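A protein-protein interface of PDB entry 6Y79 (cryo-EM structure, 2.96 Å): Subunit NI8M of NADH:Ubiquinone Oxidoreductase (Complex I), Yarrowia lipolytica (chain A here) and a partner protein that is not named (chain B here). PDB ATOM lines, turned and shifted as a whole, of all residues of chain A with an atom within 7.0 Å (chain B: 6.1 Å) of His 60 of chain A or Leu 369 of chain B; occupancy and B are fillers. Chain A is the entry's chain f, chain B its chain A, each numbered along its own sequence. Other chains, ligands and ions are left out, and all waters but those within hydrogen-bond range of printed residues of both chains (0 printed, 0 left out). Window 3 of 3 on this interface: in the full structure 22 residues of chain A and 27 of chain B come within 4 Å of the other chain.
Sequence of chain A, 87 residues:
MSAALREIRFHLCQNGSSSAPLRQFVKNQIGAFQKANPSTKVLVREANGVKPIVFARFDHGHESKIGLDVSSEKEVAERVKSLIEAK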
ATOM      1  N   ARG A  57      15.936  31.590  11.399  1.00  0.00           N
ATOM      2  CA  ARG A  57      15.557  30.496  12.275  1.00  0.00           C
ATOM      3  C   ARG A  57      14.770  29.512  11.434  1.00  0.00           C
ATOM      4  O   ARG A  57      13.681  29.849  10.958  1.00  0.00           O
ATOM      5  CB  ARG A  57      14.682  31.014  13.423  1.00  0.00           C
ATOM      6  CG  ARG A  57      14.749  30.255  14.729  1.00  0.00           C
ATOM      7  CD  ARG A  57      13.663  29.183  14.918  1.00  0.00           C
ATOM      8  NE  ARG A  57      12.273  29.576  14.654  1.00  0.00           N
ATOM      9  CZ  ARG A  57      11.534  30.354  15.442  1.00  0.00           C
ATOM     10  NH1 ARG A  57      10.274  30.618  15.122  1.00  0.00           N
ATOM     11  NH2 ARG A  57      12.053  30.890  16.538  1.00  0.00           N
ATOM     12  N   PHE A  58      15.322  28.317  11.241  1.00  0.00           N
ATOM     13  CA  PHE A  58      14.635  27.227  10.576  1.00  0.00           C
ATOM     14  C   PHE A  58      13.927  26.387  11.632  1.00  0.00           C
ATOM     15  O   PHE A  58      13.901  26.736  12.813  1.00  0.00           O
ATOM     16  CB  PHE A  58      15.630  26.426   9.739  1.00  0.00           C
ATOM     17  CG  PHE A  58      16.203  27.206   8.604  1.00  0.00           C
ATOM     18  CD1 PHE A  58      15.440  27.464   7.481  1.00  0.00           C
ATOM     19  CD2 PHE A  58      17.491  27.711   8.669  1.00  0.00           C
ATOM     20  CE1 PHE A  58      15.950  28.196   6.437  1.00  0.00           C
ATOM     21  CE2 PHE A  58      18.010  28.445   7.625  1.00  0.00           C
ATOM     22  CZ  PHE A  58      17.237  28.686   6.506  1.00  0.00           C
ATOM     23  N   ASP A  59      13.348  25.264  11.222  1.00  0.00           N
ATOM     24  CA  ASP A  59      12.461  24.553  12.131  1.00  0.00           C
ATOM     25  C   ASP A  59      13.233  23.660  13.100  1.00  0.00           C
ATOM     26  O   ASP A  59      14.333  23.186  12.805  1.00  0.00           O
ATOM     27  CB  ASP A  59      11.422  23.765  11.333  1.00  0.00           C
ATOM     28  CG  ASP A  59      10.390  24.678  10.698  1.00  0.00           C
ATOM     29  OD1 ASP A  59      10.200  25.797  11.226  1.00  0.00           O
ATOM     30  OD2 ASP A  59       9.753  24.282   9.700  1.00  0.00           O
ATOM     31  N   HIS A  60      12.618  23.462  14.276  1.00  0.00           N
ATOM     32  CA  HIS A  60      13.206  22.837  15.471  1.00  0.00           C
ATOM     33  C   HIS A  60      14.448  23.584  15.957  1.00  0.00           C
ATOM     34  O   HIS A  60      15.447  22.983  16.362  1.00  0.00           O
ATOM     35  CB  HIS A  60      13.471  21.346  15.265  1.00  0.00           C
ATOM     36  CG  HIS A  60      12.213  20.543  15.181  1.00  0.00           C
ATOM     37  ND1 HIS A  60      11.498  20.422  14.011  1.00  0.00           N
ATOM     38  CD2 HIS A  60      11.514  19.866  16.122  1.00  0.00           C
ATOM     39  CE1 HIS A  60      10.422  19.686  14.229  1.00  0.00           C
ATOM     40  NE2 HIS A  60      10.409  19.333  15.502  1.00  0.00           N
ATOM     41  N   GLY A  61      14.357  24.912  15.949  1.00  0.00           N
ATOM     42  CA  GLY A  61      15.281  25.760  16.676  1.00  0.00           C
ATOM     43  C   GLY A  61      16.677  25.833  16.117  1.00  0.00           C
ATOM     44  O   GLY A  61      17.623  26.098  16.866  1.00  0.00           O
ATOM     45  N   HIS A  62      16.839  25.607  14.823  1.00  0.00           N
ATOM     46  CA  HIS A  62      18.133  25.729  14.175  1.00  0.00           C
ATOM     47  C   HIS A  62      18.166  27.060  13.438  1.00  0.00           C
ATOM     48  O   HIS A  62      17.298  27.333  12.600  1.00  0.00           O
ATOM     49  CB  HIS A  62      18.387  24.562  13.223  1.00  0.00           C
ATOM     50  CG  HIS A  62      19.750  24.575  12.608  1.00  0.00           C
ATOM     51  ND1 HIS A  62      20.878  24.163  13.284  1.00  0.00           N
ATOM     52  CD2 HIS A  62      20.169  24.953  11.376  1.00  0.00           C
ATOM     53  CE1 HIS A  62      21.932  24.285  12.497  1.00  0.00           C
ATOM     54  NE2 HIS A  62      21.529  24.765  11.334  1.00  0.00           N
ATOM     55  N   GLU A  63      19.155  27.883  13.764  1.00  0.00           N
ATOM     56  CA  GLU A  63      19.311  29.203  13.180  1.00  0.00           C
ATOM     57  C   GLU A  63      20.751  29.376  12.725  1.00  0.00           C
ATOM     58  O   GLU A  63      21.662  28.717  13.234  1.00  0.00           O
ATOM     59  CB  GLU A  63      18.942  30.301  14.192  1.00  0.00           C
ATOM     60  CG  GLU A  63      19.882  30.388  15.382  1.00  0.00           C
ATOM     61  CD  GLU A  63      19.494  31.466  16.363  1.00  0.00           C
ATOM     62  OE1 GLU A  63      18.527  32.208  16.090  1.00  0.00           O
ATOM     63  OE2 GLU A  63      20.161  31.570  17.412  1.00  0.00           O
ATOM     64  N   TYR B 336       4.467  14.731  28.242  1.00  0.00           N
ATOM     65  CA  TYR B 336       4.850  15.040  26.866  1.00  0.00           C
ATOM     66  C   TYR B 336       5.012  13.769  26.045  1.00  0.00           C
ATOM     67  O   TYR B 336       4.574  13.714  24.891  1.00  0.00           O
ATOM     68  CB  TYR B 336       6.143  15.861  26.812  1.00  0.00           C
ATOM     69  CG  TYR B 336       6.525  16.209  25.384  1.00  0.00           C
ATOM     70  CD1 TYR B 336       5.880  17.233  24.703  1.00  0.00           C
ATOM     71  CD2 TYR B 336       7.501  15.482  24.700  1.00  0.00           C
ATOM     72  CE1 TYR B 336       6.210  17.539  23.393  1.00  0.00           C
ATOM     73  CE2 TYR B 336       7.823  15.774  23.391  1.00  0.00           C
ATOM     74  CZ  TYR B 336       7.177  16.804  22.744  1.00  0.00           C
ATOM     75  OH  TYR B 336       7.500  17.093  21.439  1.00  0.00           O
ATOM     76  N   PRO B 341       2.686  15.877  21.275  1.00  0.00           N
ATOM     77  CA  PRO B 341       2.367  16.891  20.264  1.00  0.00           C
ATOM     78  C   PRO B 341       3.517  17.079  19.285  1.00  0.00           C
ATOM     79  O   PRO B 341       4.570  17.625  19.631  1.00  0.00           O
ATOM     80  CB  PRO B 341       2.090  18.156  21.096  1.00  0.00           C
ATOM     81  CG  PRO B 341       2.831  17.958  22.348  1.00  0.00           C
ATOM     82  CD  PRO B 341       2.832  16.487  22.619  1.00  0.00           C
ATOM     83  N   LYS B 342       3.325  16.603  18.056  1.00  0.00           N
ATOM     84  CA  LYS B 342       4.396  16.617  17.069  1.00  0.00           C
ATOM     85  C   LYS B 342       4.669  18.015  16.531  1.00  0.00           C
ATOM     86  O   LYS B 342       5.793  18.303  16.103  1.00  0.00           O
ATOM     87  CB  LYS B 342       4.057  15.667  15.918  1.00  0.00           C
ATOM     88  CG  LYS B 342       4.023  14.204  16.324  1.00  0.00           C
ATOM     89  CD  LYS B 342       3.846  13.293  15.119  1.00  0.00           C
ATOM     90  CE  LYS B 342       2.422  13.329  14.591  1.00  0.00           C
ATOM     91  NZ  LYS B 342       2.223  12.356  13.483  1.00  0.00           N
ATOM     92  N   PHE B 346       1.735  22.438  20.933  1.00  0.00           N
ATOM     93  CA  PHE B 346       2.298  22.860  22.211  1.00  0.00           C
ATOM     94  C   PHE B 346       2.128  24.371  22.301  1.00  0.00           C
ATOM     95  O   PHE B 346       2.973  25.143  21.847  1.00  0.00           O
ATOM     96  CB  PHE B 346       3.756  22.451  22.353  1.00  0.00           C
ATOM     97  CG  PHE B 346       4.359  22.825  23.680  1.00  0.00           C
ATOM     98  CD1 PHE B 346       4.064  22.095  24.820  1.00  0.00           C
ATOM     99  CD2 PHE B 346       5.219  23.909  23.791  1.00  0.00           C
ATOM    100  CE1 PHE B 346       4.616  22.439  26.044  1.00  0.00           C
ATOM    101  CE2 PHE B 346       5.773  24.253  25.010  1.00  0.00           C
ATOM    102  CZ  PHE B 346       5.472  23.520  26.135  1.00  0.00           C
ATOM    103  N   ASP B 364      12.611  29.948  22.857  1.00  0.00           N
ATOM    104  CA  ASP B 364      13.639  29.010  22.422  1.00  0.00           C
ATOM    105  C   ASP B 364      13.210  27.566  22.669  1.00  0.00           C
ATOM    106  O   ASP B 364      13.473  26.688  21.837  1.00  0.00           O
ATOM    107  CB  ASP B 364      14.947  29.327  23.154  1.00  0.00           C
ATOM    108  CG  ASP B 364      16.170  28.662  22.532  1.00  0.00           C
ATOM    109  OD1 ASP B 364      16.051  27.923  21.529  1.00  0.00           O
ATOM    110  OD2 ASP B 364      17.283  28.897  23.052  1.00  0.00           O
ATOM    111  N   MET B 365      12.513  27.307  23.783  1.00  0.00           N
ATOM    112  CA  MET B 365      12.074  25.944  24.071  1.00  0.00           C
ATOM    113  C   MET B 365      10.969  25.495  23.121  1.00  0.00           C
ATOM    114  O   MET B 365      10.980  24.349  22.662  1.00  0.00           O
ATOM    115  CB  MET B 365      11.602  25.826  25.522  1.00  0.00           C
ATOM    116  CG  MET B 365      11.215  24.403  25.926  1.00  0.00           C
ATOM    117  SD  MET B 365      10.680  24.253  27.639  1.00  0.00           S
ATOM    118  CE  MET B 365       9.098  25.087  27.562  1.00  0.00           C
ATOM    119  N   THR B 366      10.018  26.379  22.801  1.00  0.00           N
ATOM    120  CA  THR B 366       8.950  25.981  21.884  1.00  0.00           C
ATOM    121  C   THR B 366       9.433  25.870  20.448  1.00  0.00           C
ATOM    122  O   THR B 366       8.894  25.067  19.678  1.00  0.00           O
ATOM    123  CB  THR B 366       7.786  26.962  21.923  1.00  0.00           C
ATOM    124  OG1 THR B 366       8.240  28.262  21.524  1.00  0.00           O
ATOM    125  CG2 THR B 366       7.242  27.031  23.288  1.00  0.00           C
ATOM    126  N   ASN B 367      10.394  26.658  20.048  1.00  0.00           N
ATOM    127  CA  ASN B 367      10.809  26.617  18.658  1.00  0.00           C
ATOM    128  C   ASN B 367      11.908  25.599  18.405  1.00  0.00           C
ATOM    129  O   ASN B 367      12.060  25.147  17.267  1.00  0.00           O
ATOM    130  CB  ASN B 367      11.211  28.015  18.223  1.00  0.00           C
ATOM    131  CG  ASN B 367      10.039  28.962  18.267  1.00  0.00           C
ATOM    132  OD1 ASN B 367      10.214  30.177  18.274  1.00  0.00           O
ATOM    133  ND2 ASN B 367       8.841  28.420  18.243  1.00  0.00           N
ATOM    134  N   ALA B 368      12.669  25.218  19.439  1.00  0.00           N
ATOM    135  CA  ALA B 368      13.459  24.000  19.347  1.00  0.00           C
ATOM    136  C   ALA B 368      12.624  22.758  19.627  1.00  0.00           C
ATOM    137  O   ALA B 368      13.134  21.642  19.491  1.00  0.00           O
ATOM    138  CB  ALA B 368      14.650  24.066  20.299  1.00  0.00           C
ATOM    139  N   LEU B 369      11.359  22.934  20.014  1.00  0.00           N
ATOM    140  CA  LEU B 369      10.420  21.822  20.046  1.00  0.00           C
ATOM    141  C   LEU B 369       9.846  21.546  18.664  1.00  0.00           C
ATOM    142  O   LEU B 369       9.679  20.385  18.278  1.00  0.00           O
ATOM    143  CB  LEU B 369       9.290  22.115  21.028  1.00  0.00           C
ATOM    144  CG  LEU B 369       8.353  20.949  21.294  1.00  0.00           C
ATOM    145  CD1 LEU B 369       9.169  19.842  21.908  1.00  0.00           C
ATOM    146  CD2 LEU B 369       7.259  21.368  22.230  1.00  0.00           C
ATOM    147  N   GLY B 370       9.548  22.600  17.906  1.00  0.00           N
ATOM    148  CA  GLY B 370       8.969  22.452  16.589  1.00  0.00           C
ATOM    149  C   GLY B 370       7.521  22.891  16.508  1.00  0.00           C
ATOM    150  O   GLY B 370       6.719  22.273  15.801  1.00  0.00           O
ATOM    151  N   SER B 371       7.175  23.959  17.227  1.00  0.00           N
ATOM    152  CA  SER B 371       5.802  24.460  17.246  1.00  0.00           C
ATOM    153  C   SER B 371       5.835  25.924  17.659  1.00  0.00           C
ATOM    154  O   SER B 371       6.149  26.225  18.813  1.00  0.00           O
ATOM    155  CB  SER B 371       4.941  23.651  18.208  1.00  0.00           C
ATOM    156  OG  SER B 371       5.344  23.855  19.551  1.00  0.00           O
ATOM    157  N   GLU B 372       5.513  26.826  16.739  1.00  0.00           N
ATOM    158  CA  GLU B 372       5.382  28.231  17.120  1.00  0.00           C
ATOM    159  C   GLU B 372       3.935  28.601  17.448  1.00  0.00           C
ATOM    160  O   GLU B 372       3.433  29.662  17.070  1.00  0.00           O
ATOM    161  CB  GLU B 372       5.974  29.130  16.037  1.00  0.00           C
ATOM    162  CG  GLU B 372       7.481  29.033  15.785  1.00  0.00           C
ATOM    163  CD  GLU B 372       7.822  27.908  14.823  1.00  0.00           C
ATOM    164  OE1 GLU B 372       6.896  27.179  14.406  1.00  0.00           O
ATOM    165  OE2 GLU B 372       9.016  27.721  14.511  1.00  0.00           O
ATOM    166  N   LEU B 633      13.140  17.212  28.273  1.00  0.00           N
ATOM    167  CA  LEU B 633      12.722  17.009  26.896  1.00  0.00           C
ATOM    168  C   LEU B 633      13.965  16.786  26.030  1.00  0.00           C
ATOM    169  O   LEU B 633      15.071  16.584  26.537  1.00  0.00           O
ATOM    170  CB  LEU B 633      11.852  18.175  26.440  1.00  0.00           C
ATOM    171  CG  LEU B 633      10.555  18.208  27.254  1.00  0.00           C
ATOM    172  CD1 LEU B 633       9.683  19.392  26.879  1.00  0.00           C
ATOM    173  CD2 LEU B 633       9.791  16.895  27.113  1.00  0.00           C
ATOM    174  N   VAL B 635      15.561  18.899  24.163  1.00  0.00           N
ATOM    175  CA  VAL B 635      16.121  20.188  23.777  1.00  0.00           C
ATOM    176  C   VAL B 635      17.239  20.558  24.741  1.00  0.00           C
ATOM    177  O   VAL B 635      17.021  20.646  25.952  1.00  0.00           O
ATOM    178  CB  VAL B 635      15.039  21.278  23.761  1.00  0.00           C
ATOM    179  CG1 VAL B 635      15.663  22.637  23.534  1.00  0.00           C
ATOM    180  CG2 VAL B 635      13.989  20.972  22.701  1.00  0.00           C
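Among the printed residues, pairs that only touch across the chains: His 60 of chain A with Ala 368 of chain B, His 60 of chain A with Gly 370 of chain B, Gly 61 of chain A with Ala 368 of chain B and Asp 59 of chain A with Glu 372 of chain B.
The backbone carbonyl oxygen (O) of Asn 367 of chain B lies within hydrogen-bond range of the backbone NH (N) of Gly 61 of chain A, 2.7 Å away.
O of Asn 367 of chain B sits close to N of His 60 of chain A (3.5 Å).
OE2 of Glu 372 of chain B is in salt-bridge range of NH1 of Arg 57 of chain A (3.2 Å).
The side-chain amide oxygen of Asn 367 of chain B is in hydrogen-bond range of the guanidinium group of Arg 57 of chain A (2.6 Å).
O of Leu 369 of chain B lies close to NE2 of His 60 of chain A.
Printed residues of chain B within 4 Å of Arg 57 of chain A: Asn 367 (2.6 Å) and Glu 372 (3.2 Å).
Printed residues of chain B within 4 Å of His 60 of chain A: Asn 367, Ala 368, Leu 369 and Gly 370.
Printed residues of chain B within 4 Å of Gly 61 of chain A: Asn 367 (2.7 Å) and Ala 368 (3.6 Å).
Pro 341 of chain B touches none of the printed residues of chain A.
Of the printed residues of chain A, Asn 367 of chain B touches Arg 57 (2.6 Å), His 60 (3.1 Å) and Gly 61 (2.7 Å).
Of chain A, only His 60 comes within 4 Å of Leu 369 of chain B.
The nearest printed residue of chain B that does not touch Asp 59 of chain A is Asn 367 of chain B (4.6 Å).
Hydrophobic or aromatic side chains of chain A within 4 Å of the printed part of chain B: His 60.
Of the 15 printed residues of chain B, 5 touch a printed residue of chain A.
Printed residues of chain B that touch a printed residue of chain A: Asn 367, Ala 368, Leu 369, Gly 370 and Glu 372.
Along chain B the printed residues that touch a printed residue of chain A span positions 367 to 372.
ND2 of Asn 367 of chain B lies within hydrogen-bond range of OG1 of Thr 366 of chain B (3.3 Å).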
